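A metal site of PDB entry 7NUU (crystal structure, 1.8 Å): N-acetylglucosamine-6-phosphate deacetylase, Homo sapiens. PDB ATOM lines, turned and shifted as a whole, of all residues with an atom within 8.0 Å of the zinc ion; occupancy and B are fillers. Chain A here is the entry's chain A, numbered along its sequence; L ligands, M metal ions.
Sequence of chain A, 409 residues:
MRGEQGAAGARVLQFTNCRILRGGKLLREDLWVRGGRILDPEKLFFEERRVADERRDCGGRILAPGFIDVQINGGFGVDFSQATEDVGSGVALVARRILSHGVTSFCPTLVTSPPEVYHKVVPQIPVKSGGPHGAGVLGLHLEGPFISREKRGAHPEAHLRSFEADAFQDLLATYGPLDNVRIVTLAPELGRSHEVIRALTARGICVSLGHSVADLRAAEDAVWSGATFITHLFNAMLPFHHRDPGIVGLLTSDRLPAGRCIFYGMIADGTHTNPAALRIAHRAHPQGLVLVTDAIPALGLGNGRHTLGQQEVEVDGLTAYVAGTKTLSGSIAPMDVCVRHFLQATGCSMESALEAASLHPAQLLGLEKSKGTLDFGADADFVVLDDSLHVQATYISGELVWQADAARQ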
ATOM      1  N   GLN A  71     -12.550 -22.362  11.706  1.00  0.00           N
ATOM      2  CA  GLN A  71     -12.606 -21.088  12.429  1.00  0.00           C
ATOM      3  C   GLN A  71     -11.199 -20.775  12.946  1.00  0.00           C
ATOM      4  O   GLN A  71     -10.801 -21.252  14.016  1.00  0.00           O
ATOM      5  CB  GLN A  71     -13.628 -21.133  13.549  1.00  0.00           C
ATOM      6  CG  GLN A  71     -13.892 -19.768  14.161  1.00  0.00           C
ATOM      7  CD  GLN A  71     -15.131 -19.714  15.013  1.00  0.00           C
ATOM      8  OE1 GLN A  71     -15.881 -20.699  15.127  1.00  0.00           O
ATOM      9  NE2 GLN A  71     -15.374 -18.552  15.622  1.00  0.00           N
ATOM     10  N   ASN A  73      -8.712 -17.134  12.962  1.00  0.00           N
ATOM     11  CA  ASN A  73      -8.733 -15.709  12.664  1.00  0.00           C
ATOM     12  C   ASN A  73      -7.382 -15.164  12.224  1.00  0.00           C
ATOM     13  O   ASN A  73      -7.281 -13.994  11.865  1.00  0.00           O
ATOM     14  CB  ASN A  73      -9.205 -14.945  13.901  1.00  0.00           C
ATOM     15  CG  ASN A  73     -10.521 -15.462  14.415  1.00  0.00           C
ATOM     16  OD1 ASN A  73     -11.554 -15.283  13.777  1.00  0.00           O
ATOM     17  ND2 ASN A  73     -10.501 -16.140  15.549  1.00  0.00           N
ATOM     18  N   THR A 109     -10.898 -16.709   8.858  1.00  0.00           N
ATOM     19  CA  THR A 109     -12.067 -16.173   9.543  1.00  0.00           C
ATOM     20  C   THR A 109     -11.848 -14.703   9.852  1.00  0.00           C
ATOM     21  O   THR A 109     -10.762 -14.297  10.274  1.00  0.00           O
ATOM     22  CB  THR A 109     -12.331 -16.959  10.827  1.00  0.00           C
ATOM     23  OG1 THR A 109     -12.472 -18.347  10.506  1.00  0.00           O
ATOM     24  CG2 THR A 109     -13.599 -16.482  11.519  1.00  0.00           C
ATOM     25  N   VAL A 111     -13.543 -11.372  11.967  1.00  0.00           N
ATOM     26  CA  VAL A 111     -14.455 -10.998  13.041  1.00  0.00           C
ATOM     27  C   VAL A 111     -15.158  -9.703  12.654  1.00  0.00           C
ATOM     28  O   VAL A 111     -14.808  -9.062  11.657  1.00  0.00           O
ATOM     29  CB  VAL A 111     -13.705 -10.844  14.373  1.00  0.00           C
ATOM     30  CG1 VAL A 111     -13.102 -12.178  14.790  1.00  0.00           C
ATOM     31  CG2 VAL A 111     -12.623  -9.772  14.295  1.00  0.00           C
ATOM     32  N   HIS A 141     -14.815 -17.613   6.469  1.00  0.00           N
ATOM     33  CA  HIS A 141     -15.796 -17.684   7.547  1.00  0.00           C
ATOM     34  C   HIS A 141     -15.942 -16.262   8.090  1.00  0.00           C
ATOM     35  O   HIS A 141     -14.999 -15.708   8.656  1.00  0.00           O
ATOM     36  CB  HIS A 141     -15.308 -18.663   8.618  1.00  0.00           C
ATOM     37  CG  HIS A 141     -16.206 -18.790   9.812  1.00  0.00           C
ATOM     38  ND1 HIS A 141     -15.986 -19.733  10.794  1.00  0.00           N
ATOM     39  CD2 HIS A 141     -17.312 -18.105  10.193  1.00  0.00           C
ATOM     40  CE1 HIS A 141     -16.913 -19.620  11.721  1.00  0.00           C
ATOM     41  NE2 HIS A 141     -17.730 -18.645  11.379  1.00  0.00           N
ATOM     42  N   GLU A 143     -17.461 -14.217  10.815  1.00  0.00           N
ATOM     43  CA  GLU A 143     -18.064 -14.324  12.136  1.00  0.00           C
ATOM     44  C   GLU A 143     -18.442 -12.929  12.587  1.00  0.00           C
ATOM     45  O   GLU A 143     -17.571 -12.110  12.912  1.00  0.00           O
ATOM     46  CB  GLU A 143     -17.106 -14.981  13.136  1.00  0.00           C
ATOM     47  CG  GLU A 143     -17.832 -15.468  14.390  1.00  0.00           C
ATOM     48  CD  GLU A 143     -16.925 -15.554  15.598  1.00  0.00           C
ATOM     49  OE1 GLU A 143     -17.235 -16.361  16.503  1.00  0.00           O
ATOM     50  OE2 GLU A 143     -15.932 -14.803  15.633  1.00  0.00           O
ATOM     51  N   GLY A 144     -19.748 -12.651  12.598  1.00  0.00           N
ATOM     52  CA  GLY A 144     -20.230 -11.300  12.778  1.00  0.00           C
ATOM     53  C   GLY A 144     -20.252 -10.575  11.451  1.00  0.00           C
ATOM     54  O   GLY A 144     -19.761 -11.075  10.440  1.00  0.00           O
ATOM     55  N   ILE A 147     -24.609 -10.251  14.941  1.00  0.00           N
ATOM     56  CA  ILE A 147     -24.643 -11.022  16.169  1.00  0.00           C
ATOM     57  C   ILE A 147     -25.154 -10.125  17.291  1.00  0.00           C
ATOM     58  O   ILE A 147     -25.368  -8.919  17.108  1.00  0.00           O
ATOM     59  CB  ILE A 147     -23.254 -11.594  16.532  1.00  0.00           C
ATOM     60  CG1 ILE A 147     -22.192 -10.500  16.500  1.00  0.00           C
ATOM     61  CG2 ILE A 147     -22.887 -12.675  15.547  1.00  0.00           C
ATOM     62  CD1 ILE A 147     -20.849 -10.923  17.076  1.00  0.00           C
ATOM     63  N   LYS A 151     -23.920 -10.985  23.734  1.00  0.00           N
ATOM     64  CA  LYS A 151     -22.919 -12.037  23.633  1.00  0.00           C
ATOM     65  C   LYS A 151     -21.878 -11.702  22.574  1.00  0.00           C
ATOM     66  O   LYS A 151     -21.366 -12.581  21.875  1.00  0.00           O
ATOM     67  CB  LYS A 151     -23.587 -13.380  23.355  1.00  0.00           C
ATOM     68  CG  LYS A 151     -24.442 -13.864  24.514  1.00  0.00           C
ATOM     69  CD  LYS A 151     -23.576 -14.197  25.728  1.00  0.00           C
ATOM     70  CE  LYS A 151     -24.353 -14.872  26.825  1.00  0.00           C
ATOM     71  NZ  LYS A 151     -23.516 -15.031  28.051  1.00  0.00           N
ATOM     72  N   ARG A 152     -21.544 -10.431  22.452  1.00  0.00           N
ATOM     73  CA  ARG A 152     -20.561 -10.038  21.445  1.00  0.00           C
ATOM     74  C   ARG A 152     -19.170 -10.551  21.778  1.00  0.00           C
ATOM     75  O   ARG A 152     -18.331 -10.634  20.872  1.00  0.00           O
ATOM     76  CB  ARG A 152     -20.549  -8.523  21.299  1.00  0.00           C
ATOM     77  CG  ARG A 152     -20.082  -7.778  22.530  1.00  0.00           C
ATOM     78  CD  ARG A 152     -20.214  -6.269  22.342  1.00  0.00           C
ATOM     79  NE  ARG A 152     -19.594  -5.522  23.435  1.00  0.00           N
ATOM     80  CZ  ARG A 152     -20.215  -5.217  24.580  1.00  0.00           C
ATOM     81  NH1 ARG A 152     -21.469  -5.604  24.792  1.00  0.00           N
ATOM     82  NH2 ARG A 152     -19.574  -4.525  25.520  1.00  0.00           N
ATOM     83  N   GLY A 153     -18.905 -10.911  23.026  1.00  0.00           N
ATOM     84  CA  GLY A 153     -17.602 -11.414  23.394  1.00  0.00           C
ATOM     85  C   GLY A 153     -16.519 -10.407  23.036  1.00  0.00           C
ATOM     86  O   GLY A 153     -16.576  -9.238  23.445  1.00  0.00           O
ATOM     87  N   ALA A 154     -15.550 -10.844  22.246  1.00  0.00           N
ATOM     88  CA  ALA A 154     -14.447 -10.001  21.808  1.00  0.00           C
ATOM     89  C   ALA A 154     -14.803  -9.139  20.595  1.00  0.00           C
ATOM     90  O   ALA A 154     -13.931  -8.424  20.099  1.00  0.00           O
ATOM     91  CB  ALA A 154     -13.223 -10.850  21.465  1.00  0.00           C
ATOM     92  N   HIS A 155     -16.029  -9.209  20.101  1.00  0.00           N
ATOM     93  CA  HIS A 155     -16.419  -8.402  18.944  1.00  0.00           C
ATOM     94  C   HIS A 155     -16.820  -7.005  19.391  1.00  0.00           C
ATOM     95  O   HIS A 155     -17.586  -6.869  20.357  1.00  0.00           O
ATOM     96  CB  HIS A 155     -17.574  -9.087  18.211  1.00  0.00           C
ATOM     97  CG  HIS A 155     -17.204 -10.422  17.662  1.00  0.00           C
ATOM     98  ND1 HIS A 155     -17.158 -10.691  16.303  1.00  0.00           N
ATOM     99  CD2 HIS A 155     -16.808 -11.560  18.282  1.00  0.00           C
ATOM    100  CE1 HIS A 155     -16.765 -11.932  16.123  1.00  0.00           C
ATOM    101  NE2 HIS A 155     -16.553 -12.488  17.300  1.00  0.00           N
ATOM    102  N   THR A 185     -21.339 -16.781  10.537  1.00  0.00           N
ATOM    103  CA  THR A 185     -21.934 -16.898  11.864  1.00  0.00           C
ATOM    104  C   THR A 185     -22.794 -15.677  12.115  1.00  0.00           C
ATOM    105  O   THR A 185     -22.357 -14.539  11.956  1.00  0.00           O
ATOM    106  CB  THR A 185     -20.878 -16.991  12.971  1.00  0.00           C
ATOM    107  OG1 THR A 185     -20.159 -18.215  12.841  1.00  0.00           O
ATOM    108  CG2 THR A 185     -21.529 -16.910  14.363  1.00  0.00           C
ATOM    109  N   GLY A 210     -24.314 -18.313  16.444  1.00  0.00           N
ATOM    110  CA  GLY A 210     -23.361 -18.004  17.487  1.00  0.00           C
ATOM    111  C   GLY A 210     -23.487 -16.575  17.970  1.00  0.00           C
ATOM    112  O   GLY A 210     -24.187 -15.757  17.368  1.00  0.00           O
ATOM    113  N   HIS A 211     -22.782 -16.300  19.058  1.00  0.00           N
ATOM    114  CA  HIS A 211     -22.795 -14.980  19.696  1.00  0.00           C
ATOM    115  C   HIS A 211     -24.231 -14.475  19.827  1.00  0.00           C
ATOM    116  O   HIS A 211     -24.599 -13.388  19.382  1.00  0.00           O
ATOM    117  CB  HIS A 211     -21.918 -13.999  18.905  1.00  0.00           C
ATOM    118  CG  HIS A 211     -20.458 -14.313  18.985  1.00  0.00           C
ATOM    119  ND1 HIS A 211     -19.636 -13.780  19.947  1.00  0.00           N
ATOM    120  CD2 HIS A 211     -19.682 -15.140  18.238  1.00  0.00           C
ATOM    121  CE1 HIS A 211     -18.416 -14.253  19.792  1.00  0.00           C
ATOM    122  NE2 HIS A 211     -18.418 -15.094  18.762  1.00  0.00           N
ATOM    123  N   THR A 231     -21.419 -22.118  16.372  1.00  0.00           N
ATOM    124  CA  THR A 231     -20.085 -21.551  16.564  1.00  0.00           C
ATOM    125  C   THR A 231     -19.670 -21.621  18.031  1.00  0.00           C
ATOM    126  O   THR A 231     -20.374 -21.111  18.910  1.00  0.00           O
ATOM    127  CB  THR A 231     -20.056 -20.125  16.030  1.00  0.00           C
ATOM    128  OG1 THR A 231     -20.194 -20.154  14.613  1.00  0.00           O
ATOM    129  CG2 THR A 231     -18.739 -19.433  16.395  1.00  0.00           C
ATOM    130  N   HIS A 232     -18.497 -22.214  18.262  1.00  0.00           N
ATOM    131  CA  HIS A 232     -17.935 -22.563  19.564  1.00  0.00           C
ATOM    132  C   HIS A 232     -18.988 -22.726  20.661  1.00  0.00           C
ATOM    133  O   HIS A 232     -19.197 -21.846  21.507  1.00  0.00           O
ATOM    134  CB  HIS A 232     -16.831 -21.577  19.984  1.00  0.00           C
ATOM    135  CG  HIS A 232     -17.153 -20.128  19.774  1.00  0.00           C
ATOM    136  ND1 HIS A 232     -18.255 -19.521  20.327  1.00  0.00           N
ATOM    137  CD2 HIS A 232     -16.473 -19.164  19.113  1.00  0.00           C
ATOM    138  CE1 HIS A 232     -18.253 -18.239  19.997  1.00  0.00           C
ATOM    139  NE2 HIS A 232     -17.181 -17.992  19.256  1.00  0.00           N
ATOM    140  N   ASN A 235     -19.558 -21.139  24.322  1.00  0.00           N
ATOM    141  CA  ASN A 235     -18.912 -19.829  24.338  1.00  0.00           C
ATOM    142  C   ASN A 235     -19.783 -18.793  23.640  1.00  0.00           C
ATOM    143  O   ASN A 235     -20.264 -19.022  22.526  1.00  0.00           O
ATOM    144  CB  ASN A 235     -17.530 -19.894  23.679  1.00  0.00           C
ATOM    145  CG  ASN A 235     -16.608 -20.875  24.384  1.00  0.00           C
ATOM    146  OD1 ASN A 235     -15.951 -21.698  23.748  1.00  0.00           O
ATOM    147  ND2 ASN A 235     -16.552 -20.799  25.698  1.00  0.00           N
ATOM    148  N   ALA A 236     -20.027 -17.660  24.313  1.00  0.00           N
ATOM    149  CA  ALA A 236     -20.800 -16.563  23.743  1.00  0.00           C
ATOM    150  C   ALA A 236     -22.213 -17.023  23.385  1.00  0.00           C
ATOM    151  O   ALA A 236     -22.738 -16.724  22.313  1.00  0.00           O
ATOM    152  CB  ALA A 236     -20.115 -15.961  22.523  1.00  0.00           C
ATOM    153  N   ILE A 267     -13.921 -25.475  21.075  1.00  0.00           N
ATOM    154  CA  ILE A 267     -12.533 -25.065  21.259  1.00  0.00           C
ATOM    155  C   ILE A 267     -11.943 -25.903  22.378  1.00  0.00           C
ATOM    156  O   ILE A 267     -12.270 -25.709  23.550  1.00  0.00           O
ATOM    157  CB  ILE A 267     -12.430 -23.572  21.593  1.00  0.00           C
ATOM    158  CG1 ILE A 267     -13.114 -22.733  20.516  1.00  0.00           C
ATOM    159  CG2 ILE A 267     -10.967 -23.160  21.744  1.00  0.00           C
ATOM    160  CD1 ILE A 267     -13.325 -21.256  20.919  1.00  0.00           C
ATOM    161  N   HIS A 272     -11.499 -22.596  27.009  1.00  0.00           N
ATOM    162  CA  HIS A 272     -12.843 -22.210  26.597  1.00  0.00           C
ATOM    163  C   HIS A 272     -13.900 -23.157  27.129  1.00  0.00           C
ATOM    164  O   HIS A 272     -15.013 -22.723  27.404  1.00  0.00           O
ATOM    165  CB  HIS A 272     -12.914 -22.127  25.070  1.00  0.00           C
ATOM    166  CG  HIS A 272     -12.350 -20.858  24.519  1.00  0.00           C
ATOM    167  ND1 HIS A 272     -10.997 -20.630  24.408  1.00  0.00           N
ATOM    168  CD2 HIS A 272     -12.959 -19.735  24.067  1.00  0.00           C
ATOM    169  CE1 HIS A 272     -10.799 -19.422  23.905  1.00  0.00           C
ATOM    170  NE2 HIS A 272     -11.973 -18.860  23.689  1.00  0.00           N
ATOM    171  N   ASP A 294     -10.082 -21.636  16.668  1.00  0.00           N
ATOM    172  CA  ASP A 294     -10.432 -20.247  16.977  1.00  0.00           C
ATOM    173  C   ASP A 294      -9.165 -19.441  17.222  1.00  0.00           C
ATOM    174  O   ASP A 294      -9.129 -18.526  18.046  1.00  0.00           O
ATOM    175  CB  ASP A 294     -11.374 -20.179  18.171  1.00  0.00           C
ATOM    176  CG  ASP A 294     -12.082 -18.835  18.285  1.00  0.00           C
ATOM    177  OD1 ASP A 294     -12.477 -18.288  17.236  1.00  0.00           O
ATOM    178  OD2 ASP A 294     -12.281 -18.343  19.423  1.00  0.00           O
ATOM    179  N   LEU A 308      -7.158  -8.250  17.065  1.00  0.00           N
ATOM    180  CA  LEU A 308      -8.218  -9.122  16.568  1.00  0.00           C
ATOM    181  C   LEU A 308      -9.249  -8.169  15.972  1.00  0.00           C
ATOM    182  O   LEU A 308     -10.114  -7.654  16.682  1.00  0.00           O
ATOM    183  CB  LEU A 308      -8.793  -9.999  17.670  1.00  0.00           C
ATOM    184  CG  LEU A 308      -9.929 -10.923  17.234  1.00  0.00           C
ATOM    185  CD1 LEU A 308      -9.442 -11.907  16.167  1.00  0.00           C
ATOM    186  CD2 LEU A 308     -10.504 -11.668  18.437  1.00  0.00           C
ATOM    187  N   LEU A 328     -12.431 -13.576  27.125  1.00  0.00           N
ATOM    188  CA  LEU A 328     -11.704 -14.462  26.236  1.00  0.00           C
ATOM    189  C   LEU A 328     -11.778 -13.934  24.802  1.00  0.00           C
ATOM    190  O   LEU A 328     -12.835 -13.499  24.347  1.00  0.00           O
ATOM    191  CB  LEU A 328     -12.271 -15.879  26.301  1.00  0.00           C
ATOM    192  CG  LEU A 328     -11.977 -16.705  27.551  1.00  0.00           C
ATOM    193  CD1 LEU A 328     -12.592 -18.101  27.380  1.00  0.00           C
ATOM    194  CD2 LEU A 328     -10.483 -16.807  27.847  1.00  0.00           C
ATOM    195  N   GLY A 330     -10.351 -15.693  21.698  1.00  0.00           N
ATOM    196  CA  GLY A 330      -9.731 -16.678  20.839  1.00  0.00           C
ATOM    197  C   GLY A 330      -8.692 -17.489  21.576  1.00  0.00           C
ATOM    198  O   GLY A 330      -8.559 -17.433  22.801  1.00  0.00           O
HETATM  199  C1  LIG L   1     -12.643 -15.420  18.090  1.00  0.00           C
HETATM  200  O1  LIG L   1     -12.203 -14.417  18.953  1.00  0.00           O
HETATM  201  C2  LIG L   1     -13.984 -15.915  18.607  1.00  0.00           C
HETATM  202  O2  LIG L   1     -14.452 -16.974  17.842  1.00  0.00           O
HETATM  203  C3  LIG L   1     -14.975 -14.776  18.521  1.00  0.00           C
HETATM  204  O3  LIG L   1     -15.670 -14.754  19.713  1.00  0.00           O
HETATM  205 ZN    ZN M   1     -16.802 -16.186  18.333  1.00  0.00          ZN
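The side-chain carboxylate (OE1) of Glu 143 lies close to the side-chain amide nitrogen (NE2) of Gln 71 (3.0 Å). NE2 of His 155 sits at hydrogen-bond distance from OE2 of Glu 143, 2.9 Å away. O of Ala 236 sits close to N of His 211, at 3.3 Å. A ring nitrogen (ND1) of His 232 is in hydrogen-bond range of the backbone carbonyl oxygen of Asn 235 (3.0 Å). A ring nitrogen (ND1) of His 211 is in hydrogen-bond range of the backbone carbonyl oxygen (O) of Lys 151 (2.9 Å). The backbone NH of Asp 294 sits at hydrogen-bond distance from the backbone carbonyl oxygen of Gln 71, at 2.8 Å.
Gln 71 touches the zinc ion (NE2 to ZN, 3.9 Å). NE2 of His 155 touches the zinc ion, at 3.8 Å.
The zinc ion is bound by the side-chain carboxylate of Glu 143 (1.9 Å), a ring nitrogen (NE2) of His 211 (2.0 Å), a ring nitrogen (NE2) of His 232 (2.1 Å), an oxygen (O3) of the ligand (2.3 Å) and an oxygen (O2) of the ligand (2.5 Å). The zinc ion has five donor atoms within binding distance.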
